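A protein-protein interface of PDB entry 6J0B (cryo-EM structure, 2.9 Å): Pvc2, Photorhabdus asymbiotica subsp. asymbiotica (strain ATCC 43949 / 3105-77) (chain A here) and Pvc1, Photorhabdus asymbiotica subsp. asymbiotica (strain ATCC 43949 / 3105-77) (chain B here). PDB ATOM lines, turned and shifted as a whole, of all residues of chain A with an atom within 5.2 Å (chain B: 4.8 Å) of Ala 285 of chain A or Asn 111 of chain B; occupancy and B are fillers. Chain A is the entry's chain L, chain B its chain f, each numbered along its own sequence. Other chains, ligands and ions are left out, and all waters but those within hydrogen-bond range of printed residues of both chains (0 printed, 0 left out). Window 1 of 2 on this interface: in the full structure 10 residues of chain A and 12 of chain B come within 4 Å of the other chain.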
ATOM      1  N   TRP A 280      32.477 -22.515  22.303  1.00  0.00           N
ATOM      2  CA  TRP A 280      31.543 -23.618  22.081  1.00  0.00           C
ATOM      3  C   TRP A 280      30.755 -23.971  23.332  1.00  0.00           C
ATOM      4  O   TRP A 280      29.609 -24.415  23.233  1.00  0.00           O
ATOM      5  CB  TRP A 280      32.290 -24.858  21.603  1.00  0.00           C
ATOM      6  CG  TRP A 280      33.108 -24.660  20.387  1.00  0.00           C
ATOM      7  CD1 TRP A 280      32.911 -23.742  19.407  1.00  0.00           C
ATOM      8  CD2 TRP A 280      34.269 -25.403  20.017  1.00  0.00           C
ATOM      9  NE1 TRP A 280      33.877 -23.865  18.443  1.00  0.00           N
ATOM     10  CE2 TRP A 280      34.725 -24.880  18.796  1.00  0.00           C
ATOM     11  CE3 TRP A 280      34.969 -26.460  20.601  1.00  0.00           C
ATOM     12  CZ2 TRP A 280      35.849 -25.377  18.149  1.00  0.00           C
ATOM     13  CZ3 TRP A 280      36.083 -26.951  19.957  1.00  0.00           C
ATOM     14  CH2 TRP A 280      36.512 -26.411  18.746  1.00  0.00           C
ATOM     15  N   GLU A 281      31.341 -23.792  24.508  1.00  0.00           N
ATOM     16  CA  GLU A 281      30.600 -24.037  25.733  1.00  0.00           C
ATOM     17  C   GLU A 281      29.721 -22.865  26.123  1.00  0.00           C
ATOM     18  O   GLU A 281      28.940 -22.983  27.070  1.00  0.00           O
ATOM     19  CB  GLU A 281      31.564 -24.362  26.861  1.00  0.00           C
ATOM     20  CG  GLU A 281      32.616 -25.373  26.465  1.00  0.00           C
ATOM     21  CD  GLU A 281      32.166 -26.793  26.657  1.00  0.00           C
ATOM     22  OE1 GLU A 281      32.899 -27.711  26.234  1.00  0.00           O
ATOM     23  OE2 GLU A 281      31.085 -26.993  27.238  1.00  0.00           O
ATOM     24  N   ARG A 282      29.840 -21.743  25.423  1.00  0.00           N
ATOM     25  CA  ARG A 282      28.901 -20.645  25.562  1.00  0.00           C
ATOM     26  C   ARG A 282      27.798 -20.716  24.523  1.00  0.00           C
ATOM     27  O   ARG A 282      26.683 -20.252  24.776  1.00  0.00           O
ATOM     28  CB  ARG A 282      29.643 -19.316  25.443  1.00  0.00           C
ATOM     29  CG  ARG A 282      28.987 -18.182  26.169  1.00  0.00           C
ATOM     30  CD  ARG A 282      30.039 -17.304  26.788  1.00  0.00           C
ATOM     31  NE  ARG A 282      30.925 -16.722  25.790  1.00  0.00           N
ATOM     32  CZ  ARG A 282      30.776 -15.503  25.284  1.00  0.00           C
ATOM     33  NH1 ARG A 282      29.773 -14.736  25.686  1.00  0.00           N
ATOM     34  NH2 ARG A 282      31.631 -15.051  24.377  1.00  0.00           N
ATOM     35  N   VAL A 283      28.098 -21.290  23.358  1.00  0.00           N
ATOM     36  CA  VAL A 283      27.077 -21.551  22.353  1.00  0.00           C
ATOM     37  C   VAL A 283      26.135 -22.647  22.827  1.00  0.00           C
ATOM     38  O   VAL A 283      24.914 -22.546  22.668  1.00  0.00           O
ATOM     39  CB  VAL A 283      27.748 -21.912  21.015  1.00  0.00           C
ATOM     40  CG1 VAL A 283      26.733 -22.310  19.996  1.00  0.00           C
ATOM     41  CG2 VAL A 283      28.533 -20.744  20.496  1.00  0.00           C
ATOM     42  N   ARG A 284      26.684 -23.698  23.440  1.00  0.00           N
ATOM     43  CA  ARG A 284      25.853 -24.796  23.921  1.00  0.00           C
ATOM     44  C   ARG A 284      25.019 -24.375  25.117  1.00  0.00           C
ATOM     45  O   ARG A 284      23.868 -24.798  25.253  1.00  0.00           O
ATOM     46  CB  ARG A 284      26.717 -25.993  24.296  1.00  0.00           C
ATOM     47  CG  ARG A 284      25.929 -27.264  24.489  1.00  0.00           C
ATOM     48  CD  ARG A 284      26.786 -28.326  25.107  1.00  0.00           C
ATOM     49  NE  ARG A 284      27.443 -27.805  26.294  1.00  0.00           N
ATOM     50  CZ  ARG A 284      28.383 -28.451  26.967  1.00  0.00           C
ATOM     51  NH1 ARG A 284      28.934 -27.896  28.038  1.00  0.00           N
ATOM     52  NH2 ARG A 284      28.782 -29.647  26.562  1.00  0.00           N
ATOM     53  N   ALA A 285      25.583 -23.548  25.994  1.00  0.00           N
ATOM     54  CA  ALA A 285      24.845 -23.101  27.166  1.00  0.00           C
ATOM     55  C   ALA A 285      23.721 -22.153  26.792  1.00  0.00           C
ATOM     56  O   ALA A 285      22.686 -22.138  27.458  1.00  0.00           O
ATOM     57  CB  ALA A 285      25.789 -22.433  28.160  1.00  0.00           C
ATOM     58  N   ALA A 286      23.891 -21.377  25.723  1.00  0.00           N
ATOM     59  CA  ALA A 286      22.845 -20.451  25.307  1.00  0.00           C
ATOM     60  C   ALA A 286      21.673 -21.183  24.674  1.00  0.00           C
ATOM     61  O   ALA A 286      20.521 -20.768  24.828  1.00  0.00           O
ATOM     62  CB  ALA A 286      23.411 -19.427  24.336  1.00  0.00           C
ATOM     63  N   ILE A 287      21.948 -22.265  23.949  1.00  0.00           N
ATOM     64  CA  ILE A 287      20.876 -23.056  23.356  1.00  0.00           C
ATOM     65  C   ILE A 287      20.183 -23.894  24.419  1.00  0.00           C
ATOM     66  O   ILE A 287      18.956 -24.047  24.404  1.00  0.00           O
ATOM     67  CB  ILE A 287      21.437 -23.925  22.219  1.00  0.00           C
ATOM     68  CG1 ILE A 287      22.017 -23.041  21.125  1.00  0.00           C
ATOM     69  CG2 ILE A 287      20.373 -24.830  21.631  1.00  0.00           C
ATOM     70  CD1 ILE A 287      22.535 -23.821  19.982  1.00  0.00           C
ATOM     71  N   SER A 288      20.950 -24.419  25.378  1.00  0.00           N
ATOM     72  CA  SER A 288      20.385 -25.307  26.388  1.00  0.00           C
ATOM     73  C   SER A 288      19.465 -24.562  27.344  1.00  0.00           C
ATOM     74  O   SER A 288      18.535 -25.156  27.896  1.00  0.00           O
ATOM     75  CB  SER A 288      21.499 -25.996  27.168  1.00  0.00           C
ATOM     76  OG  SER A 288      22.439 -26.583  26.291  1.00  0.00           O
ATOM     77  N   ASN A 289      19.709 -23.268  27.561  1.00  0.00           N
ATOM     78  CA  ASN A 289      18.775 -22.462  28.341  1.00  0.00           C
ATOM     79  C   ASN A 289      17.471 -22.276  27.592  1.00  0.00           C
ATOM     80  O   ASN A 289      16.388 -22.323  28.185  1.00  0.00           O
ATOM     81  CB  ASN A 289      19.367 -21.093  28.660  1.00  0.00           C
ATOM     82  CG  ASN A 289      20.613 -21.170  29.492  1.00  0.00           C
ATOM     83  OD1 ASN A 289      21.493 -20.330  29.377  1.00  0.00           O
ATOM     84  ND2 ASN A 289      20.710 -22.190  30.323  1.00  0.00           N
ATOM     85  N   ILE B  94      24.495 -16.510  33.137  1.00  0.00           N
ATOM     86  CA  ILE B  94      25.844 -16.426  33.680  1.00  0.00           C
ATOM     87  C   ILE B  94      26.442 -17.820  33.600  1.00  0.00           C
ATOM     88  O   ILE B  94      25.776 -18.800  33.942  1.00  0.00           O
ATOM     89  CB  ILE B  94      25.831 -15.886  35.126  1.00  0.00           C
ATOM     90  CG1 ILE B  94      25.866 -14.359  35.146  1.00  0.00           C
ATOM     91  CG2 ILE B  94      26.992 -16.404  35.954  1.00  0.00           C
ATOM     92  CD1 ILE B  94      24.541 -13.699  34.921  1.00  0.00           C
ATOM     93  N   THR B  95      27.662 -17.927  33.082  1.00  0.00           N
ATOM     94  CA  THR B  95      28.372 -19.197  33.042  1.00  0.00           C
ATOM     95  C   THR B  95      29.709 -19.051  33.747  1.00  0.00           C
ATOM     96  O   THR B  95      30.509 -18.187  33.385  1.00  0.00           O
ATOM     97  CB  THR B  95      28.616 -19.685  31.610  1.00  0.00           C
ATOM     98  OG1 THR B  95      29.654 -18.904  31.014  1.00  0.00           O
ATOM     99  CG2 THR B  95      27.362 -19.583  30.756  1.00  0.00           C
ATOM    100  N   THR B 109      32.005 -26.626  33.970  1.00  0.00           N
ATOM    101  CA  THR B 109      31.173 -25.497  33.577  1.00  0.00           C
ATOM    102  C   THR B 109      29.888 -25.514  34.387  1.00  0.00           C
ATOM    103  O   THR B 109      29.216 -26.545  34.461  1.00  0.00           O
ATOM    104  CB  THR B 109      30.848 -25.531  32.077  1.00  0.00           C
ATOM    105  OG1 THR B 109      32.059 -25.540  31.316  1.00  0.00           O
ATOM    106  CG2 THR B 109      30.039 -24.316  31.669  1.00  0.00           C
ATOM    107  N   TRP B 110      29.562 -24.381  34.996  1.00  0.00           N
ATOM    108  CA  TRP B 110      28.278 -24.150  35.635  1.00  0.00           C
ATOM    109  C   TRP B 110      27.482 -23.168  34.791  1.00  0.00           C
ATOM    110  O   TRP B 110      28.046 -22.268  34.174  1.00  0.00           O
ATOM    111  CB  TRP B 110      28.457 -23.603  37.052  1.00  0.00           C
ATOM    112  CG  TRP B 110      28.923 -24.626  38.029  1.00  0.00           C
ATOM    113  CD1 TRP B 110      28.159 -25.292  38.932  1.00  0.00           C
ATOM    114  CD2 TRP B 110      30.258 -25.109  38.201  1.00  0.00           C
ATOM    115  NE1 TRP B 110      28.932 -26.158  39.659  1.00  0.00           N
ATOM    116  CE2 TRP B 110      30.227 -26.064  39.228  1.00  0.00           C
ATOM    117  CE3 TRP B 110      31.480 -24.821  37.587  1.00  0.00           C
ATOM    118  CZ2 TRP B 110      31.364 -26.736  39.654  1.00  0.00           C
ATOM    119  CZ3 TRP B 110      32.604 -25.488  38.012  1.00  0.00           C
ATOM    120  CH2 TRP B 110      32.540 -26.436  39.032  1.00  0.00           C
ATOM    121  N   ASN B 111      26.168 -23.356  34.746  1.00  0.00           N
ATOM    122  CA  ASN B 111      25.295 -22.500  33.956  1.00  0.00           C
ATOM    123  C   ASN B 111      24.163 -22.004  34.832  1.00  0.00           C
ATOM    124  O   ASN B 111      23.518 -22.796  35.521  1.00  0.00           O
ATOM    125  CB  ASN B 111      24.724 -23.235  32.747  1.00  0.00           C
ATOM    126  CG  ASN B 111      25.793 -23.752  31.828  1.00  0.00           C
ATOM    127  OD1 ASN B 111      26.773 -23.066  31.554  1.00  0.00           O
ATOM    128  ND2 ASN B 111      25.619 -24.974  31.348  1.00  0.00           N
ATOM    129  N   VAL B 112      23.925 -20.698  34.806  1.00  0.00           N
ATOM    130  CA  VAL B 112      22.852 -20.071  35.565  1.00  0.00           C
ATOM    131  C   VAL B 112      21.896 -19.426  34.576  1.00  0.00           C
ATOM    132  O   VAL B 112      22.331 -18.764  33.630  1.00  0.00           O
ATOM    133  CB  VAL B 112      23.386 -19.024  36.555  1.00  0.00           C
ATOM    134  CG1 VAL B 112      22.516 -18.985  37.746  1.00  0.00           C
ATOM    135  CG2 VAL B 112      24.780 -19.346  36.974  1.00  0.00           C
ATOM    136  N   SER B 113      20.603 -19.617  34.793  1.00  0.00           N
ATOM    137  CA  SER B 113      19.578 -19.109  33.895  1.00  0.00           C
ATOM    138  C   SER B 113      18.829 -17.963  34.552  1.00  0.00           C
ATOM    139  O   SER B 113      18.566 -18.001  35.757  1.00  0.00           O
ATOM    140  CB  SER B 113      18.592 -20.210  33.516  1.00  0.00           C
ATOM    141  OG  SER B 113      19.251 -21.285  32.879  1.00  0.00           O
ATOM    142  N   ARG B 143      17.913 -22.564  38.265  1.00  0.00           N
ATOM    143  CA  ARG B 143      18.527 -23.629  37.469  1.00  0.00           C
ATOM    144  C   ARG B 143      20.041 -23.429  37.314  1.00  0.00           C
ATOM    145  O   ARG B 143      20.547 -22.942  36.303  1.00  0.00           O
ATOM    146  CB  ARG B 143      17.847 -23.798  36.106  1.00  0.00           C
ATOM    147  CG  ARG B 143      18.367 -25.018  35.364  1.00  0.00           C
ATOM    148  CD  ARG B 143      17.289 -25.883  34.857  1.00  0.00           C
ATOM    149  NE  ARG B 143      17.780 -27.130  34.282  1.00  0.00           N
ATOM    150  CZ  ARG B 143      18.292 -27.257  33.061  1.00  0.00           C
ATOM    151  NH1 ARG B 143      18.698 -28.447  32.647  1.00  0.00           N
ATOM    152  NH2 ARG B 143      18.414 -26.208  32.257  1.00  0.00           N
ATOM    153  N   VAL B 144      20.743 -23.706  38.401  1.00  0.00           N
ATOM    154  CA  VAL B 144      22.157 -24.038  38.289  1.00  0.00           C
ATOM    155  C   VAL B 144      22.269 -25.461  37.773  1.00  0.00           C
ATOM    156  O   VAL B 144      21.721 -26.391  38.372  1.00  0.00           O
ATOM    157  CB  VAL B 144      22.872 -23.891  39.631  1.00  0.00           C
ATOM    158  CG1 VAL B 144      24.327 -24.272  39.492  1.00  0.00           C
ATOM    159  CG2 VAL B 144      22.762 -22.514  40.054  1.00  0.00           C
ATOM    160  N   ILE B 145      22.965 -25.636  36.658  1.00  0.00           N
ATOM    161  CA  ILE B 145      23.352 -26.957  36.191  1.00  0.00           C
ATOM    162  C   ILE B 145      24.861 -26.975  36.019  1.00  0.00           C
ATOM    163  O   ILE B 145      25.477 -25.949  35.716  1.00  0.00           O
ATOM    164  CB  ILE B 145      22.643 -27.363  34.883  1.00  0.00           C
ATOM    165  CG1 ILE B 145      22.905 -26.355  33.771  1.00  0.00           C
ATOM    166  CG2 ILE B 145      21.163 -27.523  35.118  1.00  0.00           C
ATOM    167  CD1 ILE B 145      22.860 -26.964  32.400  1.00  0.00           C
ATOM    168  N   GLN B 147      28.032 -28.786  34.074  1.00  0.00           N
ATOM    169  CA  GLN B 147      28.351 -29.508  32.853  1.00  0.00           C
ATOM    170  C   GLN B 147      29.789 -29.994  32.893  1.00  0.00           C
ATOM    171  O   GLN B 147      30.691 -29.261  33.302  1.00  0.00           O
ATOM    172  CB  GLN B 147      28.143 -28.630  31.621  1.00  0.00           C
ATOM    173  CG  GLN B 147      26.754 -28.699  31.028  1.00  0.00           C
ATOM    174  CD  GLN B 147      26.581 -29.873  30.083  1.00  0.00           C
ATOM    175  OE1 GLN B 147      27.506 -30.655  29.866  1.00  0.00           O
ATOM    176  NE2 GLN B 147      25.392 -29.995  29.509  1.00  0.00           N
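The side-chain amide nitrogen of Asn 289 of chain A is in hydrogen-bond range of the side-chain hydroxyl of Ser 113 of chain B (3.1 Å).
OE2 of Glu 281 of chain A is in salt-bridge range of NH1 of Arg 284 of chain A (2.5 Å).
The backbone carbonyl oxygen (O) of Arg 284 of chain A sits at hydrogen-bond distance from the side-chain hydroxyl (OG) of Ser 288 of chain A, 2.5 Å away.
The side-chain amide oxygen (OD1) of Asn 289 of chain A sits close to the backbone carbonyl oxygen (O) of Ala 285 of chain A (2.9 Å).
The backbone NH (N) of Gln 147 of chain B is in hydrogen-bond range of the backbone carbonyl oxygen (O) of Thr 109 of chain B, 2.6 Å away.
N of Asn 111 of chain B is in hydrogen-bond range of O of Ile 145 of chain B (2.9 Å).
Among the printed residues, pairs that only touch across the chains: Ala 285 of chain A with Asn 111 of chain B (3.6 Å) and Arg 284 of chain A with Gln 147 of chain B (3.6 Å).
Of chain B, only Asn 111 comes within 4 Å of Ala 285 of chain A.
Printed residues of chain A within 4 Å of Asn 111 of chain B: Ala 285 (3.6 Å).
Of the printed residues of chain A, Gln 147 of chain B touches Arg 284 (3.6 Å).
Printed residues of chain A within 4 Å of Ser 113 of chain B: Asn 289 (3.1 Å).
Printed residues of chain B within 4 Å of Arg 284 of chain A: Gln 147 (3.6 Å).
The nearest residue of chain B that does not touch Ala 285 of chain A is Thr 95 of chain B (4.2 Å).
The nearest residue of chain A that does not touch Asn 111 of chain B is Asn 289 of chain A (4.8 Å).
The nearest printed residue of chain B that does not touch Arg 284 of chain A is Thr 109 of chain B (5.1 Å).
Printed residues of chain B that touch a printed residue of chain A: Asn 111, Ser 113 and Gln 147.
Of the 10 printed residues of chain A, 3 touch a printed residue of chain B.
Among the printed residues, 3 pairs touch across the chains.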
